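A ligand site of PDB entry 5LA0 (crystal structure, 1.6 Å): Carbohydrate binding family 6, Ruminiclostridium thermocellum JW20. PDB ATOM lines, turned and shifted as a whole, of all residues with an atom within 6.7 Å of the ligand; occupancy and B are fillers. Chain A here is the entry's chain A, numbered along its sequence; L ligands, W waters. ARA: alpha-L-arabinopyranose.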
ATOM      1  N   TYR A  31     -14.436  29.582 -17.192  1.00  0.00           N
ATOM      2  CA  TYR A  31     -13.402  28.574 -17.419  1.00  0.00           C
ATOM      3  C   TYR A  31     -12.044  29.109 -17.808  1.00  0.00           C
ATOM      4  O   TYR A  31     -11.887  30.231 -18.207  1.00  0.00           O
ATOM      5  CB  TYR A  31     -13.828  27.507 -18.460  1.00  0.00           C
ATOM      6  CG  TYR A  31     -13.628  27.932 -19.916  1.00  0.00           C
ATOM      7  CD1 TYR A  31     -14.577  28.744 -20.530  1.00  0.00           C
ATOM      8  CD2 TYR A  31     -12.514  27.576 -20.630  1.00  0.00           C
ATOM      9  CE1 TYR A  31     -14.387  29.210 -21.811  1.00  0.00           C
ATOM     10  CE2 TYR A  31     -12.340  28.004 -21.969  1.00  0.00           C
ATOM     11  CZ  TYR A  31     -13.301  28.790 -22.536  1.00  0.00           C
ATOM     12  OH  TYR A  31     -13.160  29.215 -23.821  1.00  0.00           O
ATOM     13  N   SER A  33      -8.046  27.093 -19.304  1.00  0.00           N
ATOM     14  CA  SER A  33      -7.406  25.868 -19.781  1.00  0.00           C
ATOM     15  C   SER A  33      -5.905  25.921 -19.552  1.00  0.00           C
ATOM     16  O   SER A  33      -5.247  26.953 -19.748  1.00  0.00           O
ATOM     17  CB  SER A  33      -7.645  25.715 -21.285  1.00  0.00           C
ATOM     18  OG  SER A  33      -6.840  24.706 -21.853  1.00  0.00           O
ATOM     19  N   GLU A  35      -4.359  23.187 -21.064  1.00  0.00           N
ATOM     20  CA  GLU A  35      -4.128  22.109 -22.058  1.00  0.00           C
ATOM     21  C   GLU A  35      -2.896  22.310 -22.923  1.00  0.00           C
ATOM     22  O   GLU A  35      -2.228  21.355 -23.288  1.00  0.00           O
ATOM     23  CB  GLU A  35      -5.358  21.873 -22.936  1.00  0.00           C
ATOM     24  CG  GLU A  35      -6.567  21.419 -22.121  1.00  0.00           C
ATOM     25  CD  GLU A  35      -7.835  21.627 -22.904  1.00  0.00           C
ATOM     26  OE1 GLU A  35      -8.242  22.803 -23.040  1.00  0.00           O
ATOM     27  OE2 GLU A  35      -8.381  20.622 -23.390  1.00  0.00           O
ATOM     28  N   TRP A  36      -2.594  23.548 -23.221  1.00  0.00           N
ATOM     29  CA  TRP A  36      -1.432  23.882 -24.005  1.00  0.00           C
ATOM     30  C   TRP A  36      -0.881  25.275 -23.729  1.00  0.00           C
ATOM     31  O   TRP A  36       0.042  25.707 -24.398  1.00  0.00           O
ATOM     32  CB  TRP A  36      -1.731  23.714 -25.492  1.00  0.00           C
ATOM     33  CG  TRP A  36      -2.721  24.723 -26.014  1.00  0.00           C
ATOM     34  CD1 TRP A  36      -2.465  26.023 -26.469  1.00  0.00           C
ATOM     35  CD2 TRP A  36      -4.089  24.501 -26.170  1.00  0.00           C
ATOM     36  NE1 TRP A  36      -3.629  26.607 -26.849  1.00  0.00           N
ATOM     37  CE2 TRP A  36      -4.645  25.698 -26.703  1.00  0.00           C
ATOM     38  CE3 TRP A  36      -4.923  23.411 -25.923  1.00  0.00           C
ATOM     39  CZ2 TRP A  36      -5.997  25.839 -26.925  1.00  0.00           C
ATOM     40  CZ3 TRP A  36      -6.265  23.548 -26.154  1.00  0.00           C
ATOM     41  CH2 TRP A  36      -6.798  24.749 -26.661  1.00  0.00           C
ATOM     42  N   TYR A  59     -10.146  23.046 -17.826  1.00  0.00           N
ATOM     43  CA  TYR A  59      -9.793  22.017 -18.782  1.00  0.00           C
ATOM     44  C   TYR A  59      -8.265  21.854 -18.629  1.00  0.00           C
ATOM     45  O   TYR A  59      -7.497  22.684 -19.087  1.00  0.00           O
ATOM     46  CB  TYR A  59     -10.218  22.364 -20.246  1.00  0.00           C
ATOM     47  CG  TYR A  59     -11.687  22.641 -20.376  1.00  0.00           C
ATOM     48  CD1 TYR A  59     -12.184  23.909 -20.123  1.00  0.00           C
ATOM     49  CD2 TYR A  59     -12.594  21.642 -20.739  1.00  0.00           C
ATOM     50  CE1 TYR A  59     -13.530  24.177 -20.230  1.00  0.00           C
ATOM     51  CE2 TYR A  59     -13.949  21.879 -20.840  1.00  0.00           C
ATOM     52  CZ  TYR A  59     -14.431  23.151 -20.594  1.00  0.00           C
ATOM     53  OH  TYR A  59     -15.789  23.414 -20.643  1.00  0.00           O
ATOM     54  N   GLU A  61      -5.837  19.130 -19.096  1.00  0.00           N
ATOM     55  CA  GLU A  61      -5.035  18.530 -20.170  1.00  0.00           C
ATOM     56  C   GLU A  61      -5.989  18.001 -21.204  1.00  0.00           C
ATOM     57  O   GLU A  61      -7.135  17.692 -20.864  1.00  0.00           O
ATOM     58  CB  GLU A  61      -4.164  17.419 -19.609  1.00  0.00           C
ATOM     59  CG  GLU A  61      -3.018  17.906 -18.766  1.00  0.00           C
ATOM     60  CD  GLU A  61      -2.190  16.782 -18.132  1.00  0.00           C
ATOM     61  OE1 GLU A  61      -2.458  15.561 -18.348  1.00  0.00           O
ATOM     62  OE2 GLU A  61      -1.227  17.152 -17.387  1.00  0.00           O
ATOM     63  N   CYS A  62      -5.562  17.984 -22.472  1.00  0.00           N
ATOM     64  CA  CYS A  62      -6.283  17.447 -23.584  1.00  0.00           C
ATOM     65  C   CYS A  62      -5.850  15.995 -23.796  1.00  0.00           C
ATOM     66  O   CYS A  62      -4.614  15.763 -23.932  1.00  0.00           O
ATOM     67  CB  CYS A  62      -5.948  18.278 -24.814  1.00  0.00           C
ATOM     68  SG  CYS A  62      -6.791  17.753 -26.296  1.00  0.00           S
ATOM     69  N   ILE A 100     -10.747  16.700 -17.911  1.00  0.00           N
ATOM     70  CA  ILE A 100      -9.959  16.334 -19.089  1.00  0.00           C
ATOM     71  C   ILE A 100     -10.720  16.931 -20.248  1.00  0.00           C
ATOM     72  O   ILE A 100     -11.911  16.733 -20.357  1.00  0.00           O
ATOM     73  CB  ILE A 100      -9.863  14.795 -19.262  1.00  0.00           C
ATOM     74  CG1 ILE A 100      -9.155  14.177 -18.074  1.00  0.00           C
ATOM     75  CG2 ILE A 100      -9.235  14.442 -20.603  1.00  0.00           C
ATOM     76  CD1 ILE A 100      -9.200  12.668 -18.036  1.00  0.00           C
ATOM     77  N   GLY A 101     -10.021  17.683 -21.096  1.00  0.00           N
ATOM     78  CA  GLY A 101     -10.564  18.247 -22.338  1.00  0.00           C
ATOM     79  C   GLY A 101     -10.269  17.353 -23.538  1.00  0.00           C
ATOM     80  O   GLY A 101      -9.558  16.349 -23.408  1.00  0.00           O
ATOM     81  N   ASN A 102     -10.787  17.752 -24.699  1.00  0.00           N
ATOM     82  CA  ASN A 102     -10.838  16.855 -25.835  1.00  0.00           C
ATOM     83  C   ASN A 102     -10.206  17.400 -27.083  1.00  0.00           C
ATOM     84  O   ASN A 102      -9.955  16.608 -28.016  1.00  0.00           O
ATOM     85  CB  ASN A 102     -12.277  16.491 -26.233  1.00  0.00           C
ATOM     86  CG  ASN A 102     -13.140  16.050 -25.082  1.00  0.00           C
ATOM     87  OD1 ASN A 102     -13.322  16.776 -24.100  1.00  0.00           O
ATOM     88  ND2 ASN A 102     -13.729  14.888 -25.212  1.00  0.00           N
ATOM     89  N   GLY A 103     -10.002  18.716 -27.178  1.00  0.00           N
ATOM     90  CA  GLY A 103      -9.438  19.267 -28.429  1.00  0.00           C
ATOM     91  C   GLY A 103     -10.289  19.004 -29.664  1.00  0.00           C
ATOM     92  O   GLY A 103     -11.459  19.353 -29.709  1.00  0.00           O
ATOM     93  N   ALA A 104      -9.705  18.357 -30.673  1.00  0.00           N
ATOM     94  CA  ALA A 104     -10.395  17.992 -31.896  1.00  0.00           C
ATOM     95  C   ALA A 104     -11.314  16.770 -31.738  1.00  0.00           C
ATOM     96  O   ALA A 104     -11.919  16.334 -32.705  1.00  0.00           O
ATOM     97  CB  ALA A 104      -9.393  17.715 -32.993  1.00  0.00           C
ATOM     98  N   ASN A 105     -11.410  16.213 -30.529  1.00  0.00           N
ATOM     99  CA  ASN A 105     -12.122  14.992 -30.300  1.00  0.00           C
ATOM    100  C   ASN A 105     -13.218  15.098 -29.247  1.00  0.00           C
ATOM    101  O   ASN A 105     -13.378  14.194 -28.410  1.00  0.00           O
ATOM    102  CB  ASN A 105     -11.105  13.908 -29.892  1.00  0.00           C
ATOM    103  CG  ASN A 105     -10.038  13.680 -30.961  1.00  0.00           C
ATOM    104  OD1 ASN A 105      -8.816  13.857 -30.735  1.00  0.00           O
ATOM    105  ND2 ASN A 105     -10.480  13.326 -32.114  1.00  0.00           N
ATOM    106  N   ASN A 106     -13.977  16.195 -29.286  1.00  0.00           N
ATOM    107  CA  ASN A 106     -15.195  16.263 -28.486  1.00  0.00           C
ATOM    108  C   ASN A 106     -16.114  15.125 -28.894  1.00  0.00           C
ATOM    109  O   ASN A 106     -16.130  14.703 -30.061  1.00  0.00           O
ATOM    110  CB  ASN A 106     -15.857  17.599 -28.637  1.00  0.00           C
ATOM    111  CG  ASN A 106     -15.190  18.695 -27.812  1.00  0.00           C
ATOM    112  OD1 ASN A 106     -14.697  18.489 -26.701  1.00  0.00           O
ATOM    113  ND2 ASN A 106     -15.215  19.898 -28.342  1.00  0.00           N
ATOM    114  N   ASN A 137     -14.572  15.541 -19.946  1.00  0.00           N
ATOM    115  CA  ASN A 137     -15.450  16.364 -20.760  1.00  0.00           C
ATOM    116  C   ASN A 137     -16.062  15.542 -21.918  1.00  0.00           C
ATOM    117  O   ASN A 137     -15.357  14.708 -22.510  1.00  0.00           O
ATOM    118  CB  ASN A 137     -14.658  17.524 -21.327  1.00  0.00           C
ATOM    119  CG  ASN A 137     -15.509  18.501 -22.050  1.00  0.00           C
ATOM    120  OD1 ASN A 137     -16.403  19.082 -21.456  1.00  0.00           O
ATOM    121  ND2 ASN A 137     -15.306  18.652 -23.347  1.00  0.00           N
ATOM    122  N   GLU A 138     -17.351  15.760 -22.233  1.00  0.00           N
ATOM    123  CA  GLU A 138     -18.045  15.279 -23.458  1.00  0.00           C
ATOM    124  C   GLU A 138     -17.429  14.004 -24.077  1.00  0.00           C
ATOM    125  O   GLU A 138     -16.858  14.062 -25.167  1.00  0.00           O
ATOM    126  CB  GLU A 138     -18.129  16.390 -24.509  1.00  0.00           C
ATOM    127  CG  GLU A 138     -18.803  17.679 -24.012  1.00  0.00           C
ATOM    128  CD  GLU A 138     -19.076  18.724 -25.044  1.00  0.00           C
ATOM    129  OE1 GLU A 138     -18.586  18.592 -26.178  1.00  0.00           O
ATOM    130  OE2 GLU A 138     -19.780  19.730 -24.702  1.00  0.00           O
ATOM    131  N   TYR A 222     -25.924  22.287 -24.572  1.00  0.00           N
ATOM    132  CA  TYR A 222     -26.064  22.278 -26.033  1.00  0.00           C
ATOM    133  C   TYR A 222     -27.391  21.694 -26.624  1.00  0.00           C
ATOM    134  O   TYR A 222     -27.629  21.805 -27.858  1.00  0.00           O
ATOM    135  CB  TYR A 222     -24.792  21.673 -26.708  1.00  0.00           C
ATOM    136  CG  TYR A 222     -23.595  22.486 -26.367  1.00  0.00           C
ATOM    137  CD1 TYR A 222     -23.404  23.749 -26.961  1.00  0.00           C
ATOM    138  CD2 TYR A 222     -22.669  22.087 -25.382  1.00  0.00           C
ATOM    139  CE1 TYR A 222     -22.342  24.553 -26.638  1.00  0.00           C
ATOM    140  CE2 TYR A 222     -21.602  22.884 -25.038  1.00  0.00           C
ATOM    141  CZ  TYR A 222     -21.439  24.120 -25.650  1.00  0.00           C
ATOM    142  OH  TYR A 222     -20.383  24.952 -25.325  1.00  0.00           O
ATOM    143  N   GLU A 246     -20.685  23.429 -18.699  1.00  0.00           N
ATOM    144  CA  GLU A 246     -20.320  24.180 -19.919  1.00  0.00           C
ATOM    145  C   GLU A 246     -21.578  24.529 -20.718  1.00  0.00           C
ATOM    146  O   GLU A 246     -22.320  23.643 -21.140  1.00  0.00           O
ATOM    147  CB  GLU A 246     -19.421  23.369 -20.850  1.00  0.00           C
ATOM    148  CG  GLU A 246     -18.810  24.193 -21.944  1.00  0.00           C
ATOM    149  CD  GLU A 246     -18.133  23.381 -23.010  1.00  0.00           C
ATOM    150  OE1 GLU A 246     -17.220  22.609 -22.645  1.00  0.00           O
ATOM    151  OE2 GLU A 246     -18.498  23.511 -24.186  1.00  0.00           O
ATOM    152  N   PHE A 277     -19.276  29.018 -20.376  1.00  0.00           N
ATOM    153  CA  PHE A 277     -18.198  28.825 -21.359  1.00  0.00           C
ATOM    154  C   PHE A 277     -17.677  30.162 -21.911  1.00  0.00           C
ATOM    155  O   PHE A 277     -17.633  30.381 -23.121  1.00  0.00           O
ATOM    156  CB  PHE A 277     -18.673  27.888 -22.479  1.00  0.00           C
ATOM    157  CG  PHE A 277     -17.551  27.263 -23.298  1.00  0.00           C
ATOM    158  CD1 PHE A 277     -16.484  26.594 -22.689  1.00  0.00           C
ATOM    159  CD2 PHE A 277     -17.587  27.303 -24.672  1.00  0.00           C
ATOM    160  CE1 PHE A 277     -15.495  25.985 -23.419  1.00  0.00           C
ATOM    161  CE2 PHE A 277     -16.604  26.678 -25.426  1.00  0.00           C
ATOM    162  CZ  PHE A 277     -15.551  26.028 -24.808  1.00  0.00           C
ATOM    163  N   VAL A 285     -10.924  29.460 -26.121  1.00  0.00           N
ATOM    164  CA  VAL A 285     -11.440  28.994 -27.432  1.00  0.00           C
ATOM    165  C   VAL A 285     -12.826  29.597 -27.762  1.00  0.00           C
ATOM    166  O   VAL A 285     -13.383  29.343 -28.826  1.00  0.00           O
ATOM    167  CB  VAL A 285     -11.530  27.423 -27.532  1.00  0.00           C
ATOM    168  CG1 VAL A 285     -10.137  26.760 -27.441  1.00  0.00           C
ATOM    169  CG2 VAL A 285     -12.463  26.869 -26.487  1.00  0.00           C
HETATM  170  C1  ARA L   1     -13.735  22.018 -25.309  1.00  0.00           C
HETATM  171  C2  ARA L   1     -12.488  21.163 -25.581  1.00  0.00           C
HETATM  172  C3  ARA L   1     -11.253  21.572 -24.799  1.00  0.00           C
HETATM  173  C4  ARA L   1     -11.058  23.102 -24.867  1.00  0.00           C
HETATM  174  C5  ARA L   1     -12.378  23.750 -24.422  1.00  0.00           C
HETATM  175  O1  ARA L   1     -14.754  21.754 -26.280  1.00  0.00           O
HETATM  176  O2  ARA L   1     -12.764  19.803 -25.350  1.00  0.00           O
HETATM  177  O3  ARA L   1     -10.151  20.857 -25.364  1.00  0.00           O
HETATM  178  O4  ARA L   1     -10.733  23.537 -26.226  1.00  0.00           O
HETATM  179  O5  ARA L   1     -13.383  23.396 -25.400  1.00  0.00           O
HETATM  180  O   HOH W   1     -16.775  20.758 -24.549  1.00  0.00           O
HETATM  181  O   HOH W   2     -12.772  23.922 -28.240  1.00  0.00           O
HETATM  182  O   HOH W   3     -15.308  24.527 -28.223  1.00  0.00           O
HETATM  183  O   HOH W   4     -17.481  23.223 -26.570  1.00  0.00           O
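C of Gly 101 touches O2 of the ligand (3.9 Å). Phe 277 touches the ligand (CZ to O5, 3.5 Å). Val 285 touches the ligand (CG1 to O4, 3.5 Å). Hydrophobic or aromatic side chains that line the ligand: Phe 277 and Val 285. Eight residues have an atom within 4 Å of the ligand: Glu 35, Gly 101, Asn 102, Gly 103, Asn 106, Asn 137, Phe 277 and Val 285.
Water W1 lies within hydrogen-bond range of the side-chain carboxylate (OE1) of Glu 246 (2.7 Å), the side-chain amide nitrogen (ND2) of Asn 137 (2.8 Å), an oxygen (O1) of the ligand (2.8 Å) and the side-chain carboxylate (OE2) of Glu 138 (3.2 Å). Water W4 lies within hydrogen-bond range of OE2 of Glu 246 (2.6 Å) and O1 of the ligand (3.1 Å).
OE1 of Glu 35 lies within hydrogen-bond range of OG of Ser 33, 2.6 Å away. The side-chain amide oxygen (OD1) of Asn 106 lies within hydrogen-bond range of the side-chain amide nitrogen (ND2) of Asn 137 (3.4 Å). N of Gly 103 is in hydrogen-bond range of SG of Cys 62 (3.5 Å). OD1 of Asn 102 lies within hydrogen-bond range of ND2 of Asn 137 (2.8 Å). The side-chain amide nitrogen of Asn 102 is in hydrogen-bond range of the backbone carbonyl oxygen of Glu 138. O of Ile 100 is in hydrogen-bond range of N of Asn 137, 2.9 Å away. The side-chain hydroxyl of Tyr 31 sits at hydrogen-bond distance from the backbone NH of Val 285, 3.2 Å away. The backbone NH of Gly 101 is in hydrogen-bond range of the backbone carbonyl oxygen of Glu 61 (2.9 Å).
The side-chain carboxylate (OE2) of Glu 35 is in hydrogen-bond range of an oxygen (O3) of the ligand (2.7 Å). O2 of the ligand is in hydrogen-bond range of OD1 of Asn 106. N of Gly 103 sits at hydrogen-bond distance from O3 of the ligand. The backbone NH (N) of Asn 102 lies within hydrogen-bond range of an oxygen (O2) of the ligand. The side-chain amide oxygen (OD1) of Asn 102 sits at hydrogen-bond distance from an oxygen (O2) of the ligand (3.3 Å). The side-chain amide nitrogen of Asn 137 is in hydrogen-bond range of an oxygen (O2) of the ligand (3.4 Å).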
